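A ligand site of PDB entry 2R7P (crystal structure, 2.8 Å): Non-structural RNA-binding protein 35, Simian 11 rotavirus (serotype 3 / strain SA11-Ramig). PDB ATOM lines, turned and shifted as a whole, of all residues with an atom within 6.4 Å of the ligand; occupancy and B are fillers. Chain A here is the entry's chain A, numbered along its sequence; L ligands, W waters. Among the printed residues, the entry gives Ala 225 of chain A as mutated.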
ATOM      1  N   VAL A 106       1.718 -24.838  15.588  1.00  0.00           N
ATOM      2  CA  VAL A 106       1.164 -25.277  14.313  1.00  0.00           C
ATOM      3  C   VAL A 106       1.123 -24.123  13.329  1.00  0.00           C
ATOM      4  O   VAL A 106       1.292 -22.962  13.708  1.00  0.00           O
ATOM      5  CB  VAL A 106      -0.277 -25.815  14.462  1.00  0.00           C
ATOM      6  CG1 VAL A 106      -0.271 -27.104  15.254  1.00  0.00           C
ATOM      7  CG2 VAL A 106      -1.160 -24.769  15.131  1.00  0.00           C
ATOM      8  N   SER A 107       0.893 -24.454  12.051  1.00  0.00           N
ATOM      9  CA  SER A 107       0.784 -23.456  10.990  1.00  0.00           C
ATOM     10  C   SER A 107      -0.703 -23.120  10.795  1.00  0.00           C
ATOM     11  O   SER A 107      -1.496 -23.976  10.392  1.00  0.00           O
ATOM     12  CB  SER A 107       1.363 -23.976   9.676  1.00  0.00           C
ATOM     13  OG  SER A 107       1.053 -23.083   8.615  1.00  0.00           O
ATOM     14  N   ILE A 108      -1.052 -21.874  11.079  1.00  0.00           N
ATOM     15  CA  ILE A 108      -2.440 -21.430  10.965  1.00  0.00           C
ATOM     16  C   ILE A 108      -2.965 -21.457   9.549  1.00  0.00           C
ATOM     17  O   ILE A 108      -4.113 -21.817   9.319  1.00  0.00           O
ATOM     18  CB  ILE A 108      -2.602 -20.012  11.571  1.00  0.00           C
ATOM     19  CG1 ILE A 108      -2.271 -20.048  13.071  1.00  0.00           C
ATOM     20  CG2 ILE A 108      -4.033 -19.532  11.396  1.00  0.00           C
ATOM     21  CD1 ILE A 108      -2.363 -18.704  13.734  1.00  0.00           C
ATOM     22  N   ARG A 109      -2.115 -21.107   8.589  1.00  0.00           N
ATOM     23  CA  ARG A 109      -2.549 -21.108   7.207  1.00  0.00           C
ATOM     24  C   ARG A 109      -2.966 -22.506   6.790  1.00  0.00           C
ATOM     25  O   ARG A 109      -3.935 -22.674   6.041  1.00  0.00           O
ATOM     26  CB  ARG A 109      -1.439 -20.578   6.302  1.00  0.00           C
ATOM     27  CG  ARG A 109      -1.056 -19.134   6.616  1.00  0.00           C
ATOM     28  CD  ARG A 109      -0.017 -18.607   5.644  1.00  0.00           C
ATOM     29  NE  ARG A 109       0.676 -17.414   6.140  1.00  0.00           N
ATOM     30  CZ  ARG A 109       1.347 -17.350   7.290  1.00  0.00           C
ATOM     31  NH1 ARG A 109       1.403 -18.421   8.076  1.00  0.00           N
ATOM     32  NH2 ARG A 109       1.963 -16.234   7.643  1.00  0.00           N
ATOM     33  N   HIS A 110      -2.247 -23.519   7.284  1.00  0.00           N
ATOM     34  CA  HIS A 110      -2.563 -24.905   6.975  1.00  0.00           C
ATOM     35  C   HIS A 110      -3.917 -25.249   7.587  1.00  0.00           C
ATOM     36  O   HIS A 110      -4.747 -25.932   6.973  1.00  0.00           O
ATOM     37  CB  HIS A 110      -1.461 -25.845   7.519  1.00  0.00           C
ATOM     38  CG  HIS A 110      -1.603 -27.276   7.068  1.00  0.00           C
ATOM     39  ND1 HIS A 110      -0.576 -27.980   6.498  1.00  0.00           N
ATOM     40  CD2 HIS A 110      -2.671 -28.115   7.104  1.00  0.00           C
ATOM     41  CE1 HIS A 110      -0.995 -29.205   6.200  1.00  0.00           C
ATOM     42  NE2 HIS A 110      -2.263 -29.309   6.556  1.00  0.00           N
ATOM     43  N   GLU A 147       1.648 -36.113   4.957  1.00  0.00           N
ATOM     44  CA  GLU A 147       0.653 -35.393   4.182  1.00  0.00           C
ATOM     45  C   GLU A 147       0.771 -35.742   2.708  1.00  0.00           C
ATOM     46  O   GLU A 147       1.834 -35.606   2.098  1.00  0.00           O
ATOM     47  CB  GLU A 147       0.814 -33.891   4.394  1.00  0.00           C
ATOM     48  CG  GLU A 147       0.018 -33.030   3.411  1.00  0.00           C
ATOM     49  CD  GLU A 147       0.203 -31.542   3.639  1.00  0.00           C
ATOM     50  OE1 GLU A 147       1.261 -31.153   4.193  1.00  0.00           O
ATOM     51  OE2 GLU A 147      -0.703 -30.768   3.249  1.00  0.00           O
ATOM     52  N   GLU A 153      -3.426 -29.743   2.612  1.00  0.00           N
ATOM     53  CA  GLU A 153      -4.087 -28.565   3.146  1.00  0.00           C
ATOM     54  C   GLU A 153      -5.009 -27.933   2.105  1.00  0.00           C
ATOM     55  O   GLU A 153      -5.872 -27.113   2.435  1.00  0.00           O
ATOM     56  CB  GLU A 153      -3.085 -27.534   3.666  1.00  0.00           C
ATOM     57  CG  GLU A 153      -2.081 -27.051   2.651  1.00  0.00           C
ATOM     58  CD  GLU A 153      -1.102 -26.063   3.255  1.00  0.00           C
ATOM     59  OE1 GLU A 153      -1.515 -24.925   3.579  1.00  0.00           O
ATOM     60  OE2 GLU A 153       0.095 -26.420   3.417  1.00  0.00           O
ATOM     61  N   TYR A 171      -2.921 -18.306   0.550  1.00  0.00           N
ATOM     62  CA  TYR A 171      -2.623 -17.588   1.789  1.00  0.00           C
ATOM     63  C   TYR A 171      -3.013 -16.101   1.779  1.00  0.00           C
ATOM     64  O   TYR A 171      -3.306 -15.540   2.840  1.00  0.00           O
ATOM     65  CB  TYR A 171      -1.123 -17.731   2.107  1.00  0.00           C
ATOM     66  CG  TYR A 171      -0.668 -19.150   2.437  1.00  0.00           C
ATOM     67  CD1 TYR A 171       0.684 -19.496   2.452  1.00  0.00           C
ATOM     68  CD2 TYR A 171      -1.595 -20.142   2.787  1.00  0.00           C
ATOM     69  CE1 TYR A 171       1.098 -20.782   2.792  1.00  0.00           C
ATOM     70  CE2 TYR A 171      -1.193 -21.421   3.132  1.00  0.00           C
ATOM     71  CZ  TYR A 171       0.158 -21.748   3.134  1.00  0.00           C
ATOM     72  OH  TYR A 171       0.552 -23.024   3.499  1.00  0.00           O
ATOM     73  N   MET A 177      -5.136 -15.348   9.249  1.00  0.00           N
ATOM     74  CA  MET A 177      -3.800 -14.763   9.236  1.00  0.00           C
ATOM     75  C   MET A 177      -3.168 -14.865   7.859  1.00  0.00           C
ATOM     76  O   MET A 177      -2.263 -15.652   7.629  1.00  0.00           O
ATOM     77  CB  MET A 177      -2.910 -15.461  10.263  1.00  0.00           C
ATOM     78  CG  MET A 177      -1.583 -14.776  10.477  1.00  0.00           C
ATOM     79  SD  MET A 177      -0.593 -15.597  11.724  1.00  0.00           S
ATOM     80  CE  MET A 177       0.583 -16.464  10.676  1.00  0.00           C
ATOM     81  N   ILE A 179      -1.118 -13.714   4.262  1.00  0.00           N
ATOM     82  CA  ILE A 179       0.207 -13.207   3.977  1.00  0.00           C
ATOM     83  C   ILE A 179      -0.063 -11.729   3.686  1.00  0.00           C
ATOM     84  O   ILE A 179      -1.012 -11.404   2.964  1.00  0.00           O
ATOM     85  CB  ILE A 179       0.801 -13.880   2.731  1.00  0.00           C
ATOM     86  CG1 ILE A 179       1.175 -15.327   3.056  1.00  0.00           C
ATOM     87  CG2 ILE A 179       2.000 -13.084   2.219  1.00  0.00           C
ATOM     88  CD1 ILE A 179       2.321 -15.456   4.039  1.00  0.00           C
ATOM     89  N   GLU A 186       3.001 -18.857  -3.836  1.00  0.00           N
ATOM     90  CA  GLU A 186       3.682 -20.089  -3.442  1.00  0.00           C
ATOM     91  C   GLU A 186       2.850 -21.298  -3.857  1.00  0.00           C
ATOM     92  O   GLU A 186       1.616 -21.242  -3.881  1.00  0.00           O
ATOM     93  CB  GLU A 186       3.908 -20.085  -1.912  1.00  0.00           C
ATOM     94  CG  GLU A 186       4.919 -21.115  -1.408  1.00  0.00           C
ATOM     95  CD  GLU A 186       5.326 -20.876   0.055  1.00  0.00           C
ATOM     96  OE1 GLU A 186       5.795 -19.768   0.383  1.00  0.00           O
ATOM     97  OE2 GLU A 186       5.193 -21.814   0.883  1.00  0.00           O
ATOM     98  N   LYS A 188       2.471 -25.837  -3.754  1.00  0.00           N
ATOM     99  CA  LYS A 188       2.789 -27.024  -2.988  1.00  0.00           C
ATOM    100  C   LYS A 188       2.477 -28.234  -3.833  1.00  0.00           C
ATOM    101  O   LYS A 188       1.406 -28.308  -4.425  1.00  0.00           O
ATOM    102  CB  LYS A 188       1.934 -27.039  -1.721  1.00  0.00           C
ATOM    103  CG  LYS A 188       2.086 -28.230  -0.804  1.00  0.00           C
ATOM    104  CD  LYS A 188       1.350 -27.954   0.490  1.00  0.00           C
ATOM    105  CE  LYS A 188       1.702 -28.981   1.541  1.00  0.00           C
ATOM    106  NZ  LYS A 188       1.079 -28.707   2.882  1.00  0.00           N
ATOM    107  N   THR A 220      11.714 -28.010  -0.450  1.00  0.00           N
ATOM    108  CA  THR A 220      10.881 -28.803   0.449  1.00  0.00           C
ATOM    109  C   THR A 220      11.253 -28.478   1.883  1.00  0.00           C
ATOM    110  O   THR A 220      12.371 -28.055   2.161  1.00  0.00           O
ATOM    111  CB  THR A 220      11.094 -30.315   0.215  1.00  0.00           C
ATOM    112  OG1 THR A 220      10.337 -31.063   1.169  1.00  0.00           O
ATOM    113  CG2 THR A 220      12.568 -30.658   0.362  1.00  0.00           C
ATOM    114  N   HIS A 221      10.305 -28.664   2.793  1.00  0.00           N
ATOM    115  CA  HIS A 221      10.571 -28.430   4.194  1.00  0.00           C
ATOM    116  C   HIS A 221      10.887 -29.768   4.836  1.00  0.00           C
ATOM    117  O   HIS A 221      11.098 -29.871   6.038  1.00  0.00           O
ATOM    118  CB  HIS A 221       9.381 -27.741   4.850  1.00  0.00           C
ATOM    119  CG  HIS A 221       9.242 -26.314   4.435  1.00  0.00           C
ATOM    120  ND1 HIS A 221       8.185 -25.511   4.819  1.00  0.00           N
ATOM    121  CD2 HIS A 221      10.032 -25.523   3.659  1.00  0.00           C
ATOM    122  CE1 HIS A 221       8.329 -24.301   4.307  1.00  0.00           C
ATOM    123  NE2 HIS A 221       9.445 -24.281   3.593  1.00  0.00           N
ATOM    124  N   GLY A 222      10.892 -30.802   3.993  1.00  0.00           N
ATOM    125  CA  GLY A 222      11.250 -32.147   4.405  1.00  0.00           C
ATOM    126  C   GLY A 222      10.187 -33.055   4.982  1.00  0.00           C
ATOM    127  O   GLY A 222      10.517 -34.143   5.463  1.00  0.00           O
ATOM    128  N   LYS A 223       8.919 -32.655   4.956  1.00  0.00           N
ATOM    129  CA  LYS A 223       7.881 -33.519   5.523  1.00  0.00           C
ATOM    130  C   LYS A 223       7.110 -34.306   4.464  1.00  0.00           C
ATOM    131  O   LYS A 223       5.970 -34.728   4.698  1.00  0.00           O
ATOM    132  CB  LYS A 223       6.898 -32.707   6.379  1.00  0.00           C
ATOM    133  CG  LYS A 223       7.524 -31.939   7.532  1.00  0.00           C
ATOM    134  CD  LYS A 223       6.563 -31.743   8.691  1.00  0.00           C
ATOM    135  CE  LYS A 223       7.016 -30.624   9.623  1.00  0.00           C
ATOM    136  NZ  LYS A 223       6.430 -29.295   9.241  1.00  0.00           N
ATOM    137  N   GLY A 224       7.725 -34.517   3.302  1.00  0.00           N
ATOM    138  CA  GLY A 224       7.059 -35.291   2.265  1.00  0.00           C
ATOM    139  C   GLY A 224       6.402 -34.531   1.117  1.00  0.00           C
ATOM    140  O   GLY A 224       5.819 -35.173   0.238  1.00  0.00           O
ATOM    141  N   ALA A 225       6.477 -33.208   1.103  1.00  0.00           N
ATOM    142  CA  ALA A 225       5.873 -32.441   0.014  1.00  0.00           C
ATOM    143  C   ALA A 225       6.769 -31.318  -0.530  1.00  0.00           C
ATOM    144  O   ALA A 225       7.556 -30.732   0.209  1.00  0.00           O
ATOM    145  CB  ALA A 225       4.539 -31.856   0.464  1.00  0.00           C
ATOM    146  N   TYR A 226       6.652 -31.028  -1.829  1.00  0.00           N
ATOM    147  CA  TYR A 226       7.459 -29.969  -2.431  1.00  0.00           C
ATOM    148  C   TYR A 226       6.805 -28.590  -2.249  1.00  0.00           C
ATOM    149  O   TYR A 226       5.580 -28.464  -2.156  1.00  0.00           O
ATOM    150  CB  TYR A 226       7.657 -30.208  -3.930  1.00  0.00           C
ATOM    151  CG  TYR A 226       8.243 -31.557  -4.275  1.00  0.00           C
ATOM    152  CD1 TYR A 226       7.427 -32.654  -4.463  1.00  0.00           C
ATOM    153  CD2 TYR A 226       9.616 -31.715  -4.415  1.00  0.00           C
ATOM    154  CE1 TYR A 226       7.946 -33.894  -4.776  1.00  0.00           C
ATOM    155  CE2 TYR A 226      10.167 -32.958  -4.729  1.00  0.00           C
ATOM    156  CZ  TYR A 226       9.327 -34.054  -4.913  1.00  0.00           C
ATOM    157  OH  TYR A 226       9.851 -35.305  -5.217  1.00  0.00           O
ATOM    158  N   ARG A 227       7.633 -27.560  -2.198  1.00  0.00           N
ATOM    159  CA  ARG A 227       7.142 -26.211  -2.047  1.00  0.00           C
ATOM    160  C   ARG A 227       7.741 -25.459  -3.222  1.00  0.00           C
ATOM    161  O   ARG A 227       8.965 -25.477  -3.411  1.00  0.00           O
ATOM    162  CB  ARG A 227       7.639 -25.601  -0.729  1.00  0.00           C
ATOM    163  CG  ARG A 227       6.669 -24.636  -0.056  1.00  0.00           C
ATOM    164  CD  ARG A 227       5.644 -25.395   0.766  1.00  0.00           C
ATOM    165  NE  ARG A 227       4.992 -24.554   1.773  1.00  0.00           N
ATOM    166  CZ  ARG A 227       4.075 -25.002   2.630  1.00  0.00           C
ATOM    167  NH1 ARG A 227       3.704 -26.271   2.610  1.00  0.00           N
ATOM    168  NH2 ARG A 227       3.521 -24.178   3.504  1.00  0.00           N
ATOM    169  N   HIS A 237      13.465 -19.306   3.549  1.00  0.00           N
ATOM    170  CA  HIS A 237      13.013 -20.670   3.717  1.00  0.00           C
ATOM    171  C   HIS A 237      14.172 -21.446   4.342  1.00  0.00           C
ATOM    172  O   HIS A 237      13.983 -22.199   5.290  1.00  0.00           O
ATOM    173  CB  HIS A 237      12.627 -21.265   2.359  1.00  0.00           C
ATOM    174  CG  HIS A 237      11.237 -20.922   1.916  1.00  0.00           C
ATOM    175  ND1 HIS A 237      10.129 -21.584   2.390  1.00  0.00           N
ATOM    176  CD2 HIS A 237      10.778 -19.966   1.077  1.00  0.00           C
ATOM    177  CE1 HIS A 237       9.045 -21.053   1.850  1.00  0.00           C
ATOM    178  NE2 HIS A 237       9.410 -20.071   1.048  1.00  0.00           N
ATOM    179  N   ARG A 240      14.343 -20.593   8.094  1.00  0.00           N
ATOM    180  CA  ARG A 240      13.239 -21.231   8.801  1.00  0.00           C
ATOM    181  C   ARG A 240      13.373 -22.746   8.953  1.00  0.00           C
ATOM    182  O   ARG A 240      13.051 -23.299  10.002  1.00  0.00           O
ATOM    183  CB  ARG A 240      11.908 -20.913   8.108  1.00  0.00           C
ATOM    184  CG  ARG A 240      11.631 -19.423   7.992  1.00  0.00           C
ATOM    185  CD  ARG A 240      10.128 -19.131   8.093  1.00  0.00           C
ATOM    186  NE  ARG A 240       9.336 -19.729   7.026  1.00  0.00           N
ATOM    187  CZ  ARG A 240       9.384 -19.357   5.747  1.00  0.00           C
ATOM    188  NH1 ARG A 240      10.183 -18.364   5.358  1.00  0.00           N
ATOM    189  NH2 ARG A 240       8.601 -19.962   4.860  1.00  0.00           N
HETATM  190  P1  LIG L   1       4.977 -28.424   4.733  1.00  0.00           P
HETATM  191  O1  LIG L   1       3.532 -28.040   4.641  1.00  0.00           O
HETATM  192  O2  LIG L   1       5.834 -27.887   3.442  1.00  0.00           O
HETATM  193  O3  LIG L   1       5.110 -30.023   4.817  1.00  0.00           O
HETATM  194  P2  LIG L   1       5.282 -26.476   7.170  1.00  0.00           P
HETATM  195  O4  LIG L   1       3.854 -26.478   7.537  1.00  0.00           O
HETATM  196  O5  LIG L   1       6.167 -26.595   8.503  1.00  0.00           O
HETATM  197  N1  LIG L   1       5.583 -27.779   6.097  1.00  0.00           N
HETATM  198  P3  LIG L   1       5.005 -23.593   6.788  1.00  0.00           P
HETATM  199  O6  LIG L   1       5.050 -22.662   5.594  1.00  0.00           O
HETATM  200  O7  LIG L   1       3.443 -23.718   7.246  1.00  0.00           O
HETATM  201  O8  LIG L   1       5.633 -25.083   6.351  1.00  0.00           O
HETATM  202  O9  LIG L   1       5.965 -22.930   7.935  1.00  0.00           O
HETATM  203  C1  LIG L   1       5.275 -22.692   9.082  1.00  0.00           C
HETATM  204  C2  LIG L   1       5.197 -21.222   9.469  1.00  0.00           C
HETATM  205  O10 LIG L   1       6.548 -20.629   9.529  1.00  0.00           O
HETATM  206  C3  LIG L   1       4.418 -20.398   8.428  1.00  0.00           C
HETATM  207  O11 LIG L   1       2.997 -20.372   8.716  1.00  0.00           O
HETATM  208  C4  LIG L   1       5.185 -19.006   8.420  1.00  0.00           C
HETATM  209  O12 LIG L   1       4.376 -17.850   8.693  1.00  0.00           O
HETATM  210  C5  LIG L   1       6.336 -19.191   9.441  1.00  0.00           C
HETATM  211  O   HOH W   1       3.883 -26.994   9.920  1.00  0.00           O
HETATM  212  O   HOH W   2       7.270 -31.038   3.042  1.00  0.00           O
HETATM  213  O   HOH W   3       2.811 -31.562   6.280  1.00  0.00           O
HETATM  214  O   HOH W   4       1.558 -24.130   5.692  1.00  0.00           O
HETATM  215  O   HOH W   5       5.042 -24.839  11.087  1.00  0.00           O
HETATM  216  O   HOH W   6       1.809 -26.685   6.121  1.00  0.00           O
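NH1 of Arg 109 lies within hydrogen-bond range of O11 of the ligand, at 2.6 Å.
O1 of the ligand lies within salt-bridge range of NH1 of Arg 227 (2.7 Å).
The side-chain amino group (NZ) of Lys 223 is in salt-bridge range of an oxygen (O5) of the ligand (2.8 Å).
OG of Ser 107 lies within hydrogen-bond range of O7 of the ligand.
O8 of the ligand is in hydrogen-bond range of ND1 of His 221 (3.0 Å).
The side-chain amino group of Lys 188 lies within salt-bridge range of an oxygen (O1) of the ligand (3.1 Å).
OE2 of Glu 153 lies within salt-bridge range of NH1 of Arg 227, at 3.7 Å.
The guanidinium group (NH2) of Arg 227 is in hydrogen-bond range of the side-chain hydroxyl (OH) of Tyr 171 (3.2 Å).
The guanidinium group of Arg 227 is in salt-bridge range of the side-chain carboxylate of Glu 186, 2.9 Å away.
OE2 of Glu 147 lies within salt-bridge range of NZ of Lys 188, 2.7 Å away.
The side-chain carboxylate (OE2) of Glu 153 is in salt-bridge range of the side-chain amino group (NZ) of Lys 188, at 2.5 Å.
The guanidinium group (NH2) of Arg 240 lies close to a ring nitrogen (ND1) of His 237.
N of Glu 153 sits at hydrogen-bond distance from OE2 of Glu 147.
OE1 of Glu 153 sits at hydrogen-bond distance from OH of Tyr 171 (2.8 Å).
Glu 147 touches the ligand (OE1 to O1, 3.9 Å).
Glu 153 touches the ligand (OE2 to O1, 3.99 Å).
NE of Arg 240 touches O10 of the ligand, 3.9 Å away.
Hydrophobic or aromatic side chains within 4 Å of the ligand: His 221.
Nine residues have an atom within 4 Å of the ligand: Ser 107, Arg 109, Glu 147, Glu 153, Lys 188, His 221, Lys 223, Arg 227 and Arg 240.
Water W1 bridges an oxygen (O4) of the ligand (2.4 Å) and the side-chain amino group (NZ) of Lys 223 (3.5 Å).
Water W4 lies within hydrogen-bond range of O7 of the ligand, OH of Tyr 171, NH2 of Arg 227 and OG of Ser 107.
Water W6 lies within hydrogen-bond range of an oxygen (O4) of the ligand (2.5 Å), a ring nitrogen (ND1) of His 110 (2.7 Å) and the side-chain carboxylate (OE2) of Glu 153 (3.2 Å).
Water W2 lies within hydrogen-bond range of O of Ala 225 (2.9 Å), O3 of the ligand (3.0 Å) and N of Lys 223 (3.0 Å).
Water W3 bridges the side-chain carboxylate of Glu 147 (2.6 Å) and an oxygen (O3) of the ligand (3.1 Å).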
